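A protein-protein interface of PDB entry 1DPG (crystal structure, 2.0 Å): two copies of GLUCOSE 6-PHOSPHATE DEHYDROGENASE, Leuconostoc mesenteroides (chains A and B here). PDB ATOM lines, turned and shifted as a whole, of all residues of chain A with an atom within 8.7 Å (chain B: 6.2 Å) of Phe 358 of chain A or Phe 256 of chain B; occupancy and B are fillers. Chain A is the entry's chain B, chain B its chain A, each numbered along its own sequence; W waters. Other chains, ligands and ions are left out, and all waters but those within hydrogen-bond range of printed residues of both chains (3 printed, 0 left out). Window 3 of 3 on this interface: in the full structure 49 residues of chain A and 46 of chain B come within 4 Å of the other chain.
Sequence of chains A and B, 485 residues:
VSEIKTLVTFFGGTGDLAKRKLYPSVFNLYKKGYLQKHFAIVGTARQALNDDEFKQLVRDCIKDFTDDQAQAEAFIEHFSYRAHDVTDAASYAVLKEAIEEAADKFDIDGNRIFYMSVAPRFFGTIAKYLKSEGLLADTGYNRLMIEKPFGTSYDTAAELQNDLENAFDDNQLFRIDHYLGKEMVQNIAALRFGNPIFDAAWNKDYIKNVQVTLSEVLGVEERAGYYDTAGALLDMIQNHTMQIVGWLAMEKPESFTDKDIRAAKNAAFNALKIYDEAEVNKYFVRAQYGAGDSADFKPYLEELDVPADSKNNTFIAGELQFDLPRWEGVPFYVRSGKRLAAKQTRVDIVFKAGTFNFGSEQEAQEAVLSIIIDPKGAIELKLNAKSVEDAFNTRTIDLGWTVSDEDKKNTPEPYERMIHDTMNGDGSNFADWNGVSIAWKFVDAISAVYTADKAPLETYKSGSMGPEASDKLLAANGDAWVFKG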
ATOM      1  N   GLY A 354       6.163 -21.770 -14.300  1.00  0.00           N
ATOM      2  CA  GLY A 354       5.699 -21.499 -15.652  1.00  0.00           C
ATOM      3  C   GLY A 354       4.614 -22.490 -16.063  1.00  0.00           C
ATOM      4  O   GLY A 354       4.414 -23.527 -15.424  1.00  0.00           O
ATOM      5  N   THR A 355       3.878 -22.166 -17.114  1.00  0.00           N
ATOM      6  CA  THR A 355       2.819 -23.050 -17.562  1.00  0.00           C
ATOM      7  C   THR A 355       3.111 -23.746 -18.906  1.00  0.00           C
ATOM      8  O   THR A 355       2.263 -24.494 -19.413  1.00  0.00           O
ATOM      9  CB  THR A 355       1.480 -22.289 -17.626  1.00  0.00           C
ATOM     10  OG1 THR A 355       1.666 -21.055 -18.342  1.00  0.00           O
ATOM     11  CG2 THR A 355       0.980 -21.998 -16.228  1.00  0.00           C
ATOM     12  N   PHE A 356       4.300 -23.505 -19.465  1.00  0.00           N
ATOM     13  CA  PHE A 356       4.716 -24.107 -20.733  1.00  0.00           C
ATOM     14  C   PHE A 356       4.755 -25.634 -20.602  1.00  0.00           C
ATOM     15  O   PHE A 356       5.353 -26.163 -19.674  1.00  0.00           O
ATOM     16  CB  PHE A 356       6.099 -23.584 -21.133  1.00  0.00           C
ATOM     17  CG  PHE A 356       6.529 -24.017 -22.504  1.00  0.00           C
ATOM     18  CD1 PHE A 356       6.076 -23.339 -23.635  1.00  0.00           C
ATOM     19  CD2 PHE A 356       7.360 -25.123 -22.676  1.00  0.00           C
ATOM     20  CE1 PHE A 356       6.448 -23.773 -24.929  1.00  0.00           C
ATOM     21  CE2 PHE A 356       7.728 -25.551 -23.943  1.00  0.00           C
ATOM     22  CZ  PHE A 356       7.273 -24.880 -25.070  1.00  0.00           C
ATOM     23  N   ASN A 357       4.095 -26.343 -21.506  1.00  0.00           N
ATOM     24  CA  ASN A 357       4.075 -27.794 -21.424  1.00  0.00           C
ATOM     25  C   ASN A 357       5.225 -28.406 -22.222  1.00  0.00           C
ATOM     26  O   ASN A 357       5.269 -28.329 -23.446  1.00  0.00           O
ATOM     27  CB  ASN A 357       2.728 -28.347 -21.904  1.00  0.00           C
ATOM     28  CG  ASN A 357       2.550 -29.814 -21.567  1.00  0.00           C
ATOM     29  OD1 ASN A 357       3.269 -30.676 -22.082  1.00  0.00           O
ATOM     30  ND2 ASN A 357       1.618 -30.106 -20.672  1.00  0.00           N
ATOM     31  N   PHE A 358       6.183 -28.974 -21.508  1.00  0.00           N
ATOM     32  CA  PHE A 358       7.323 -29.608 -22.149  1.00  0.00           C
ATOM     33  C   PHE A 358       6.981 -31.025 -22.536  1.00  0.00           C
ATOM     34  O   PHE A 358       7.683 -31.630 -23.335  1.00  0.00           O
ATOM     35  CB  PHE A 358       8.511 -29.660 -21.206  1.00  0.00           C
ATOM     36  CG  PHE A 358       9.231 -28.361 -21.068  1.00  0.00           C
ATOM     37  CD1 PHE A 358      10.021 -27.887 -22.104  1.00  0.00           C
ATOM     38  CD2 PHE A 358       9.156 -27.630 -19.883  1.00  0.00           C
ATOM     39  CE1 PHE A 358      10.738 -26.702 -21.968  1.00  0.00           C
ATOM     40  CE2 PHE A 358       9.865 -26.452 -19.733  1.00  0.00           C
ATOM     41  CZ  PHE A 358      10.662 -25.981 -20.777  1.00  0.00           C
ATOM     42  N   GLY A 359       5.908 -31.553 -21.960  1.00  0.00           N
ATOM     43  CA  GLY A 359       5.538 -32.924 -22.234  1.00  0.00           C
ATOM     44  C   GLY A 359       6.496 -33.842 -21.493  1.00  0.00           C
ATOM     45  O   GLY A 359       6.737 -34.963 -21.916  1.00  0.00           O
ATOM     46  N   SER A 360       7.035 -33.369 -20.372  1.00  0.00           N
ATOM     47  CA  SER A 360       7.973 -34.154 -19.582  1.00  0.00           C
ATOM     48  C   SER A 360       7.305 -34.744 -18.345  1.00  0.00           C
ATOM     49  O   SER A 360       6.162 -34.433 -18.033  1.00  0.00           O
ATOM     50  CB  SER A 360       9.136 -33.264 -19.148  1.00  0.00           C
ATOM     51  OG  SER A 360       8.636 -32.038 -18.624  1.00  0.00           O
ATOM     52  N   GLU A 361       8.027 -35.611 -17.651  1.00  0.00           N
ATOM     53  CA  GLU A 361       7.539 -36.244 -16.429  1.00  0.00           C
ATOM     54  C   GLU A 361       7.472 -35.188 -15.312  1.00  0.00           C
ATOM     55  O   GLU A 361       6.548 -35.166 -14.499  1.00  0.00           O
ATOM     56  CB  GLU A 361       8.516 -37.359 -16.045  1.00  0.00           C
ATOM     57  CG  GLU A 361       8.164 -38.149 -14.799  1.00  0.00           C
ATOM     58  CD  GLU A 361       9.249 -39.155 -14.427  1.00  0.00           C
ATOM     59  OE1 GLU A 361      10.108 -39.455 -15.287  1.00  0.00           O
ATOM     60  OE2 GLU A 361       9.256 -39.642 -13.272  1.00  0.00           O
ATOM     61  N   GLN A 362       8.474 -34.321 -15.282  1.00  0.00           N
ATOM     62  CA  GLN A 362       8.553 -33.264 -14.294  1.00  0.00           C
ATOM     63  C   GLN A 362       8.463 -31.948 -15.034  1.00  0.00           C
ATOM     64  O   GLN A 362       9.359 -31.603 -15.805  1.00  0.00           O
ATOM     65  CB  GLN A 362       9.892 -33.327 -13.560  1.00  0.00           C
ATOM     66  CG  GLN A 362      10.152 -32.140 -12.656  1.00  0.00           C
ATOM     67  CD  GLN A 362       9.207 -32.126 -11.486  1.00  0.00           C
ATOM     68  OE1 GLN A 362       9.300 -32.977 -10.599  1.00  0.00           O
ATOM     69  NE2 GLN A 362       8.249 -31.194 -11.494  1.00  0.00           N
ATOM     70  N   GLU A 363       7.333 -31.271 -14.891  1.00  0.00           N
ATOM     71  CA  GLU A 363       7.159 -29.966 -15.518  1.00  0.00           C
ATOM     72  C   GLU A 363       7.880 -28.905 -14.657  1.00  0.00           C
ATOM     73  O   GLU A 363       8.336 -29.205 -13.546  1.00  0.00           O
ATOM     74  CB  GLU A 363       5.670 -29.639 -15.693  1.00  0.00           C
ATOM     75  CG  GLU A 363       4.949 -30.507 -16.726  1.00  0.00           C
ATOM     76  CD  GLU A 363       5.411 -30.279 -18.177  1.00  0.00           C
ATOM     77  OE1 GLU A 363       6.221 -29.363 -18.451  1.00  0.00           O
ATOM     78  OE2 GLU A 363       4.935 -31.022 -19.061  1.00  0.00           O
ATOM     79  N   ALA A 364       7.975 -27.679 -15.169  1.00  0.00           N
ATOM     80  CA  ALA A 364       8.655 -26.580 -14.480  1.00  0.00           C
ATOM     81  C   ALA A 364       8.135 -26.309 -13.060  1.00  0.00           C
ATOM     82  O   ALA A 364       6.930 -26.266 -12.813  1.00  0.00           O
ATOM     83  CB  ALA A 364       8.583 -25.302 -15.337  1.00  0.00           C
ATOM     84  N   GLN A 365       9.061 -26.198 -12.121  1.00  0.00           N
ATOM     85  CA  GLN A 365       8.730 -25.917 -10.737  1.00  0.00           C
ATOM     86  C   GLN A 365       8.967 -24.429 -10.501  1.00  0.00           C
ATOM     87  O   GLN A 365       9.403 -23.700 -11.396  1.00  0.00           O
ATOM     88  CB  GLN A 365       9.616 -26.760  -9.820  1.00  0.00           C
ATOM     89  CG  GLN A 365       9.362 -28.234  -9.971  1.00  0.00           C
ATOM     90  CD  GLN A 365      10.399 -29.071  -9.280  1.00  0.00           C
ATOM     91  OE1 GLN A 365      11.368 -29.527  -9.904  1.00  0.00           O
ATOM     92  NE2 GLN A 365      10.218 -29.285  -7.981  1.00  0.00           N
ATOM     93  N   ASN A 384      14.914 -23.563 -13.280  1.00  0.00           N
ATOM     94  CA  ASN A 384      14.557 -24.802 -13.970  1.00  0.00           C
ATOM     95  C   ASN A 384      15.494 -24.961 -15.168  1.00  0.00           C
ATOM     96  O   ASN A 384      15.758 -24.002 -15.907  1.00  0.00           O
ATOM     97  CB  ASN A 384      13.123 -24.756 -14.507  1.00  0.00           C
ATOM     98  CG  ASN A 384      12.089 -24.722 -13.407  1.00  0.00           C
ATOM     99  OD1 ASN A 384      11.710 -25.757 -12.857  1.00  0.00           O
ATOM    100  ND2 ASN A 384      11.627 -23.527 -13.075  1.00  0.00           N
ATOM    101  N   ALA A 385      15.984 -26.173 -15.374  1.00  0.00           N
ATOM    102  CA  ALA A 385      16.866 -26.445 -16.503  1.00  0.00           C
ATOM    103  C   ALA A 385      16.523 -27.875 -16.934  1.00  0.00           C
ATOM    104  O   ALA A 385      15.494 -28.424 -16.495  1.00  0.00           O
ATOM    105  CB  ALA A 385      18.330 -26.322 -16.065  1.00  0.00           C
ATOM    106  N   LYS A 386      17.386 -28.497 -17.733  1.00  0.00           N
ATOM    107  CA  LYS A 386      17.139 -29.856 -18.195  1.00  0.00           C
ATOM    108  C   LYS A 386      17.863 -30.870 -17.308  1.00  0.00           C
ATOM    109  O   LYS A 386      18.971 -30.619 -16.836  1.00  0.00           O
ATOM    110  CB  LYS A 386      17.631 -29.991 -19.641  1.00  0.00           C
ATOM    111  CG  LYS A 386      17.416 -31.362 -20.265  1.00  0.00           C
ATOM    112  CD  LYS A 386      18.004 -31.416 -21.677  1.00  0.00           C
ATOM    113  CE  LYS A 386      17.775 -32.800 -22.318  1.00  0.00           C
ATOM    114  NZ  LYS A 386      18.352 -33.896 -21.489  1.00  0.00           N
ATOM    115  N   PHE A 392      13.823 -36.079 -22.528  1.00  0.00           N
ATOM    116  CA  PHE A 392      13.817 -34.690 -22.097  1.00  0.00           C
ATOM    117  C   PHE A 392      12.989 -34.536 -20.831  1.00  0.00           C
ATOM    118  O   PHE A 392      11.833 -34.971 -20.773  1.00  0.00           O
ATOM    119  CB  PHE A 392      13.240 -33.796 -23.178  1.00  0.00           C
ATOM    120  CG  PHE A 392      13.362 -32.351 -22.864  1.00  0.00           C
ATOM    121  CD1 PHE A 392      12.412 -31.725 -22.071  1.00  0.00           C
ATOM    122  CD2 PHE A 392      14.470 -31.636 -23.287  1.00  0.00           C
ATOM    123  CE1 PHE A 392      12.564 -30.392 -21.689  1.00  0.00           C
ATOM    124  CE2 PHE A 392      14.644 -30.309 -22.919  1.00  0.00           C
ATOM    125  CZ  PHE A 392      13.683 -29.679 -22.109  1.00  0.00           C
ATOM    126  N   ASN A 393      13.568 -33.902 -19.826  1.00  0.00           N
ATOM    127  CA  ASN A 393      12.870 -33.703 -18.562  1.00  0.00           C
ATOM    128  C   ASN A 393      13.481 -32.482 -17.894  1.00  0.00           C
ATOM    129  O   ASN A 393      14.613 -32.100 -18.232  1.00  0.00           O
ATOM    130  CB  ASN A 393      13.048 -34.932 -17.663  1.00  0.00           C
ATOM    131  CG  ASN A 393      11.926 -35.083 -16.649  1.00  0.00           C
ATOM    132  OD1 ASN A 393      10.858 -34.452 -16.766  1.00  0.00           O
ATOM    133  ND2 ASN A 393      12.148 -35.931 -15.655  1.00  0.00           N
ATOM    134  N   THR A 394      12.760 -31.868 -16.951  1.00  0.00           N
ATOM    135  CA  THR A 394      13.281 -30.689 -16.258  1.00  0.00           C
ATOM    136  C   THR A 394      13.668 -31.005 -14.827  1.00  0.00           C
ATOM    137  O   THR A 394      13.267 -32.031 -14.271  1.00  0.00           O
ATOM    138  CB  THR A 394      12.271 -29.498 -16.244  1.00  0.00           C
ATOM    139  OG1 THR A 394      11.089 -29.849 -15.504  1.00  0.00           O
ATOM    140  CG2 THR A 394      11.868 -29.126 -17.658  1.00  0.00           C
ATOM    141  N   ARG A 395      14.485 -30.132 -14.251  1.00  0.00           N
ATOM    142  CA  ARG A 395      14.926 -30.257 -12.862  1.00  0.00           C
ATOM    143  C   ARG A 395      15.298 -28.850 -12.437  1.00  0.00           C
ATOM    144  O   ARG A 395      15.465 -27.972 -13.292  1.00  0.00           O
ATOM    145  CB  ARG A 395      16.186 -31.118 -12.763  1.00  0.00           C
ATOM    146  CG  ARG A 395      17.382 -30.588 -13.583  1.00  0.00           C
ATOM    147  CD  ARG A 395      18.658 -31.298 -13.140  1.00  0.00           C
ATOM    148  NE  ARG A 395      19.850 -30.843 -13.863  1.00  0.00           N
ATOM    149  CZ  ARG A 395      21.078 -31.333 -13.650  1.00  0.00           C
ATOM    150  NH1 ARG A 395      21.249 -32.283 -12.741  1.00  0.00           N
ATOM    151  NH2 ARG A 395      22.132 -30.897 -14.338  1.00  0.00           N
ATOM    152  N   GLN B 186      20.993 -28.373 -25.168  1.00  0.00           N
ATOM    153  CA  GLN B 186      19.598 -28.725 -25.000  1.00  0.00           C
ATOM    154  C   GLN B 186      19.005 -28.113 -23.758  1.00  0.00           C
ATOM    155  O   GLN B 186      17.829 -28.260 -23.507  1.00  0.00           O
ATOM    156  CB  GLN B 186      19.435 -30.235 -24.997  1.00  0.00           C
ATOM    157  CG  GLN B 186      19.743 -30.815 -26.356  1.00  0.00           C
ATOM    158  CD  GLN B 186      19.772 -32.302 -26.360  1.00  0.00           C
ATOM    159  OE1 GLN B 186      19.186 -32.959 -25.498  1.00  0.00           O
ATOM    160  NE2 GLN B 186      20.431 -32.866 -27.369  1.00  0.00           N
ATOM    161  N   ALA B 189      16.352 -24.237 -24.282  1.00  0.00           N
ATOM    162  CA  ALA B 189      14.896 -24.141 -24.249  1.00  0.00           C
ATOM    163  C   ALA B 189      14.339 -24.311 -22.834  1.00  0.00           C
ATOM    164  O   ALA B 189      13.337 -23.685 -22.476  1.00  0.00           O
ATOM    165  CB  ALA B 189      14.251 -25.167 -25.203  1.00  0.00           C
ATOM    166  N   ALA B 190      14.971 -25.159 -22.031  1.00  0.00           N
ATOM    167  CA  ALA B 190      14.497 -25.386 -20.666  1.00  0.00           C
ATOM    168  C   ALA B 190      14.641 -24.103 -19.852  1.00  0.00           C
ATOM    169  O   ALA B 190      13.703 -23.648 -19.204  1.00  0.00           O
ATOM    170  CB  ALA B 190      15.285 -26.486 -20.022  1.00  0.00           C
ATOM    171  N   LEU B 191      15.827 -23.521 -19.910  1.00  0.00           N
ATOM    172  CA  LEU B 191      16.127 -22.287 -19.204  1.00  0.00           C
ATOM    173  C   LEU B 191      15.122 -21.183 -19.583  1.00  0.00           C
ATOM    174  O   LEU B 191      14.555 -20.501 -18.728  1.00  0.00           O
ATOM    175  CB  LEU B 191      17.556 -21.837 -19.564  1.00  0.00           C
ATOM    176  CG  LEU B 191      18.744 -21.972 -18.607  1.00  0.00           C
ATOM    177  CD1 LEU B 191      18.577 -23.130 -17.662  1.00  0.00           C
ATOM    178  CD2 LEU B 191      20.023 -22.121 -19.424  1.00  0.00           C
ATOM    179  N   ARG B 192      14.884 -21.040 -20.876  1.00  0.00           N
ATOM    180  CA  ARG B 192      14.005 -20.011 -21.367  1.00  0.00           C
ATOM    181  C   ARG B 192      12.508 -20.211 -21.127  1.00  0.00           C
ATOM    182  O   ARG B 192      11.855 -19.369 -20.506  1.00  0.00           O
ATOM    183  CB  ARG B 192      14.283 -19.789 -22.843  1.00  0.00           C
ATOM    184  CG  ARG B 192      13.290 -18.878 -23.517  1.00  0.00           C
ATOM    185  CD  ARG B 192      13.542 -18.839 -25.002  1.00  0.00           C
ATOM    186  NE  ARG B 192      12.528 -18.045 -25.684  1.00  0.00           N
ATOM    187  CZ  ARG B 192      12.403 -17.933 -27.004  1.00  0.00           C
ATOM    188  NH1 ARG B 192      13.229 -18.568 -27.827  1.00  0.00           N
ATOM    189  NH2 ARG B 192      11.457 -17.148 -27.500  1.00  0.00           N
ATOM    190  N   PHE B 193      11.962 -21.320 -21.602  1.00  0.00           N
ATOM    191  CA  PHE B 193      10.533 -21.576 -21.460  1.00  0.00           C
ATOM    192  C   PHE B 193      10.139 -22.105 -20.106  1.00  0.00           C
ATOM    193  O   PHE B 193       8.956 -22.158 -19.798  1.00  0.00           O
ATOM    194  CB  PHE B 193      10.036 -22.567 -22.526  1.00  0.00           C
ATOM    195  CG  PHE B 193      10.287 -22.118 -23.937  1.00  0.00           C
ATOM    196  CD1 PHE B 193       9.991 -20.822 -24.335  1.00  0.00           C
ATOM    197  CD2 PHE B 193      10.851 -22.988 -24.867  1.00  0.00           C
ATOM    198  CE1 PHE B 193      10.257 -20.389 -25.642  1.00  0.00           C
ATOM    199  CE2 PHE B 193      11.121 -22.554 -26.181  1.00  0.00           C
ATOM    200  CZ  PHE B 193      10.819 -21.245 -26.559  1.00  0.00           C
ATOM    201  N   GLY B 194      11.106 -22.551 -19.315  1.00  0.00           N
ATOM    202  CA  GLY B 194      10.764 -23.094 -18.013  1.00  0.00           C
ATOM    203  C   GLY B 194      10.831 -22.107 -16.853  1.00  0.00           C
ATOM    204  O   GLY B 194      10.524 -22.459 -15.709  1.00  0.00           O
ATOM    205  N   TRP B 247      18.267 -22.158 -31.917  1.00  0.00           N
ATOM    206  CA  TRP B 247      17.644 -22.411 -30.628  1.00  0.00           C
ATOM    207  C   TRP B 247      17.442 -21.103 -29.890  1.00  0.00           C
ATOM    208  O   TRP B 247      16.439 -20.915 -29.205  1.00  0.00           O
ATOM    209  CB  TRP B 247      18.523 -23.297 -29.767  1.00  0.00           C
ATOM    210  CG  TRP B 247      18.256 -24.761 -29.940  1.00  0.00           C
ATOM    211  CD1 TRP B 247      19.127 -25.709 -30.407  1.00  0.00           C
ATOM    212  CD2 TRP B 247      17.056 -25.465 -29.576  1.00  0.00           C
ATOM    213  NE1 TRP B 247      18.545 -26.957 -30.344  1.00  0.00           N
ATOM    214  CE2 TRP B 247      17.277 -26.833 -29.838  1.00  0.00           C
ATOM    215  CE3 TRP B 247      15.820 -25.072 -29.051  1.00  0.00           C
ATOM    216  CZ2 TRP B 247      16.311 -27.811 -29.589  1.00  0.00           C
ATOM    217  CZ3 TRP B 247      14.852 -26.056 -28.806  1.00  0.00           C
ATOM    218  CH2 TRP B 247      15.110 -27.406 -29.074  1.00  0.00           C
ATOM    219  N   MET B 250      14.634 -18.705 -31.880  1.00  0.00           N
ATOM    220  CA  MET B 250      13.324 -19.240 -32.160  1.00  0.00           C
ATOM    221  C   MET B 250      12.187 -18.503 -31.474  1.00  0.00           C
ATOM    222  O   MET B 250      12.355 -17.899 -30.421  1.00  0.00           O
ATOM    223  CB  MET B 250      13.259 -20.706 -31.769  1.00  0.00           C
ATOM    224  CG  MET B 250      13.413 -20.932 -30.291  1.00  0.00           C
ATOM    225  SD  MET B 250      13.291 -22.718 -29.877  1.00  0.00           S
ATOM    226  CE  MET B 250      11.592 -23.127 -30.313  1.00  0.00           C
ATOM    227  N   PRO B 253       7.055 -21.719 -29.294  1.00  0.00           N
ATOM    228  CA  PRO B 253       6.232 -22.721 -29.985  1.00  0.00           C
ATOM    229  C   PRO B 253       4.900 -23.047 -29.336  1.00  0.00           C
ATOM    230  O   PRO B 253       4.682 -22.776 -28.157  1.00  0.00           O
ATOM    231  CB  PRO B 253       7.157 -23.933 -30.019  1.00  0.00           C
ATOM    232  CG  PRO B 253       7.820 -23.845 -28.663  1.00  0.00           C
ATOM    233  CD  PRO B 253       8.137 -22.351 -28.523  1.00  0.00           C
ATOM    234  N   GLU B 254       4.011 -23.646 -30.121  1.00  0.00           N
ATOM    235  CA  GLU B 254       2.697 -24.040 -29.634  1.00  0.00           C
ATOM    236  C   GLU B 254       2.856 -25.042 -28.528  1.00  0.00           C
ATOM    237  O   GLU B 254       2.116 -25.029 -27.553  1.00  0.00           O
ATOM    238  CB  GLU B 254       1.908 -24.739 -30.708  1.00  0.00           C
ATOM    239  CG  GLU B 254       1.568 -23.924 -31.904  1.00  0.00           C
ATOM    240  CD  GLU B 254       0.438 -24.582 -32.676  1.00  0.00           C
ATOM    241  OE1 GLU B 254      -0.580 -24.927 -32.026  1.00  0.00           O
ATOM    242  OE2 GLU B 254       0.564 -24.780 -33.911  1.00  0.00           O
ATOM    243  N   SER B 255       3.760 -25.983 -28.748  1.00  0.00           N
ATOM    244  CA  SER B 255       4.042 -27.028 -27.777  1.00  0.00           C
ATOM    245  C   SER B 255       5.482 -27.453 -27.992  1.00  0.00           C
ATOM    246  O   SER B 255       6.151 -26.957 -28.900  1.00  0.00           O
ATOM    247  CB  SER B 255       3.111 -28.216 -27.990  1.00  0.00           C
ATOM    248  OG  SER B 255       3.385 -28.836 -29.234  1.00  0.00           O
ATOM    249  N   PHE B 256       5.952 -28.383 -27.181  1.00  0.00           N
ATOM    250  CA  PHE B 256       7.318 -28.813 -27.306  1.00  0.00           C
ATOM    251  C   PHE B 256       7.524 -30.070 -28.148  1.00  0.00           C
ATOM    252  O   PHE B 256       8.320 -30.923 -27.781  1.00  0.00           O
ATOM    253  CB  PHE B 256       7.949 -28.982 -25.919  1.00  0.00           C
ATOM    254  CG  PHE B 256       9.428 -28.725 -25.907  1.00  0.00           C
ATOM    255  CD1 PHE B 256       9.928 -27.496 -26.318  1.00  0.00           C
ATOM    256  CD2 PHE B 256      10.324 -29.720 -25.523  1.00  0.00           C
ATOM    257  CE1 PHE B 256      11.316 -27.251 -26.349  1.00  0.00           C
ATOM    258  CE2 PHE B 256      11.702 -29.488 -25.553  1.00  0.00           C
ATOM    259  CZ  PHE B 256      12.199 -28.249 -25.964  1.00  0.00           C
ATOM    260  N   THR B 257       6.786 -30.235 -29.241  1.00  0.00           N
ATOM    261  CA  THR B 257       7.015 -31.410 -30.092  1.00  0.00           C
ATOM    262  C   THR B 257       7.920 -30.990 -31.240  1.00  0.00           C
ATOM    263  O   THR B 257       7.942 -29.811 -31.632  1.00  0.00           O
ATOM    264  CB  THR B 257       5.734 -32.007 -30.672  1.00  0.00           C
ATOM    265  OG1 THR B 257       5.019 -30.997 -31.386  1.00  0.00           O
ATOM    266  CG2 THR B 257       4.866 -32.577 -29.571  1.00  0.00           C
ATOM    267  N   ASP B 258       8.642 -31.950 -31.803  1.00  0.00           N
ATOM    268  CA  ASP B 258       9.567 -31.646 -32.894  1.00  0.00           C
ATOM    269  C   ASP B 258       8.976 -30.801 -34.009  1.00  0.00           C
ATOM    270  O   ASP B 258       9.617 -29.870 -34.475  1.00  0.00           O
ATOM    271  CB  ASP B 258      10.275 -32.910 -33.450  1.00  0.00           C
ATOM    272  CG  ASP B 258       9.307 -33.990 -34.000  1.00  0.00           C
ATOM    273  OD1 ASP B 258       8.065 -33.819 -33.964  1.00  0.00           O
ATOM    274  OD2 ASP B 258       9.810 -35.041 -34.478  1.00  0.00           O
ATOM    275  N   ASP B 260       6.520 -28.537 -33.857  1.00  0.00           N
ATOM    276  CA  ASP B 260       6.346 -27.146 -33.444  1.00  0.00           C
ATOM    277  C   ASP B 260       7.680 -26.460 -33.231  1.00  0.00           C
ATOM    278  O   ASP B 260       7.833 -25.295 -33.591  1.00  0.00           O
ATOM    279  CB  ASP B 260       5.445 -27.047 -32.212  1.00  0.00           C
ATOM    280  CG  ASP B 260       4.001 -27.427 -32.520  1.00  0.00           C
ATOM    281  OD1 ASP B 260       3.602 -27.365 -33.701  1.00  0.00           O
ATOM    282  OD2 ASP B 260       3.259 -27.795 -31.589  1.00  0.00           O
ATOM    283  N   ILE B 261       8.660 -27.207 -32.724  1.00  0.00           N
ATOM    284  CA  ILE B 261       9.996 -26.671 -32.505  1.00  0.00           C
ATOM    285  C   ILE B 261      10.626 -26.191 -33.811  1.00  0.00           C
ATOM    286  O   ILE B 261      11.103 -25.047 -33.915  1.00  0.00           O
ATOM    287  CB  ILE B 261      10.904 -27.700 -31.818  1.00  0.00           C
ATOM    288  CG1 ILE B 261      10.396 -27.938 -30.385  1.00  0.00           C
ATOM    289  CG2 ILE B 261      12.359 -27.194 -31.824  1.00  0.00           C
ATOM    290  CD1 ILE B 261      11.064 -29.097 -29.627  1.00  0.00           C
ATOM    291  N   SER B 428      13.549 -33.146 -33.029  1.00  0.00           N
ATOM    292  CA  SER B 428      13.850 -31.970 -32.218  1.00  0.00           C
ATOM    293  C   SER B 428      15.281 -31.471 -32.297  1.00  0.00           C
ATOM    294  O   SER B 428      15.499 -30.265 -32.397  1.00  0.00           O
ATOM    295  CB  SER B 428      13.470 -32.216 -30.762  1.00  0.00           C
ATOM    296  OG  SER B 428      12.099 -32.536 -30.672  1.00  0.00           O
HETATM  297  O   HOH W   1       6.852 -23.263 -18.090  1.00  0.00           O
HETATM  298  O   HOH W   2       4.433 -30.085 -25.474  1.00  0.00           O
HETATM  299  O   HOH W   3       8.867 -22.027 -13.497  1.00  0.00           O
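O of Gly 194 of chain B sits at hydrogen-bond distance from ND2 of Asn 384 of chain A, at 3.0 Å.
The side-chain amide oxygen (OD1) of Asn 357 of chain A lies within hydrogen-bond range of the backbone NH (N) of Gly 359 of chain A (2.8 Å).
Among the printed residues, pairs that only touch across the chains: Phe 356 of chain A with Phe 193 of chain B (3.5 Å), Phe 356 of chain A with Pro 253 of chain B (3.8 Å), Phe 356 of chain A with Phe 256 of chain B (3.8 Å), Asn 357 of chain A with Phe 256 of chain B (3.7 Å), Phe 358 of chain A with Ala 189 of chain B (3.9 Å), Phe 358 of chain A with Ala 190 of chain B (3.9 Å), Phe 358 of chain A with Phe 193 of chain B (3.9 Å), Phe 358 of chain A with Gly 194 of chain B (3.8 Å), Phe 358 of chain A with Phe 256 of chain B (3.7 Å), Ala 364 of chain A with Gly 194 of chain B (3.5 Å), Asn 384 of chain A with Ala 190 of chain B (3.9 Å), Asn 384 of chain A with Leu 191 of chain B (3.4 Å), Ala 385 of chain A with Ala 190 of chain B (3.6 Å), Ala 385 of chain A with Leu 191 of chain B (3.6 Å), Lys 386 of chain A with Gln 186 of chain B (3.5 Å), Lys 386 of chain A with Ala 190 of chain B (3.7 Å), Phe 392 of chain A with Gln 186 of chain B (3.8 Å) and Phe 392 of chain A with Phe 256 of chain B (3.98 Å).
Printed residues of chain B within 4 Å of Phe 392 of chain A: Gln 186 and Phe 256.
Printed residues of chain A within 4 Å of Gln 186 of chain B: Lys 386 (3.5 Å) and Phe 392 (3.8 Å).
Trp 247 of chain B touches none of the printed residues of chain A.
Phe 256 of chain B touches just these residues of chain A: Phe 356 (3.8 Å), Asn 357 (3.7 Å), Phe 358 (3.7 Å) and Phe 392 (3.98 Å).
No residue of chain A comes within 4 Å of Thr 257 of chain B.
The nearest residue of chain B that does not touch Phe 358 of chain A is Leu 191 of chain B (5.8 Å).
The nearest residue of chain A that does not touch Phe 256 of chain B is Gly 359 of chain A (5.1 Å).
The nearest printed residue of chain B that does not touch Phe 392 of chain A is Ala 190 of chain B (4.1 Å).
Of the 19 printed residues of chain A, 8 touch a printed residue of chain B.
Along chain A the printed residues that touch a printed residue of chain B span positions 356 to 392.
Of the 18 printed residues of chain B, 8 touch a printed residue of chain A.
Hydrophobic or aromatic side chains of chain B within 4 Å of the printed part of chain A: Ala 190, Leu 191, Phe 193, Pro 253 and Phe 256.
Among the printed residues, 19 pairs touch across the chains.
No position is printed for both chains.
Of the 19 pairs that touch across the chains among the printed residues, none has its exchanged pair printed and touching as well.
Water W1 lies within hydrogen-bond range of N of Phe 356 of chain A (2.9 Å), O of Phe 193 of chain B (2.9 Å) and N of Thr 355 of chain A (3.3 Å).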
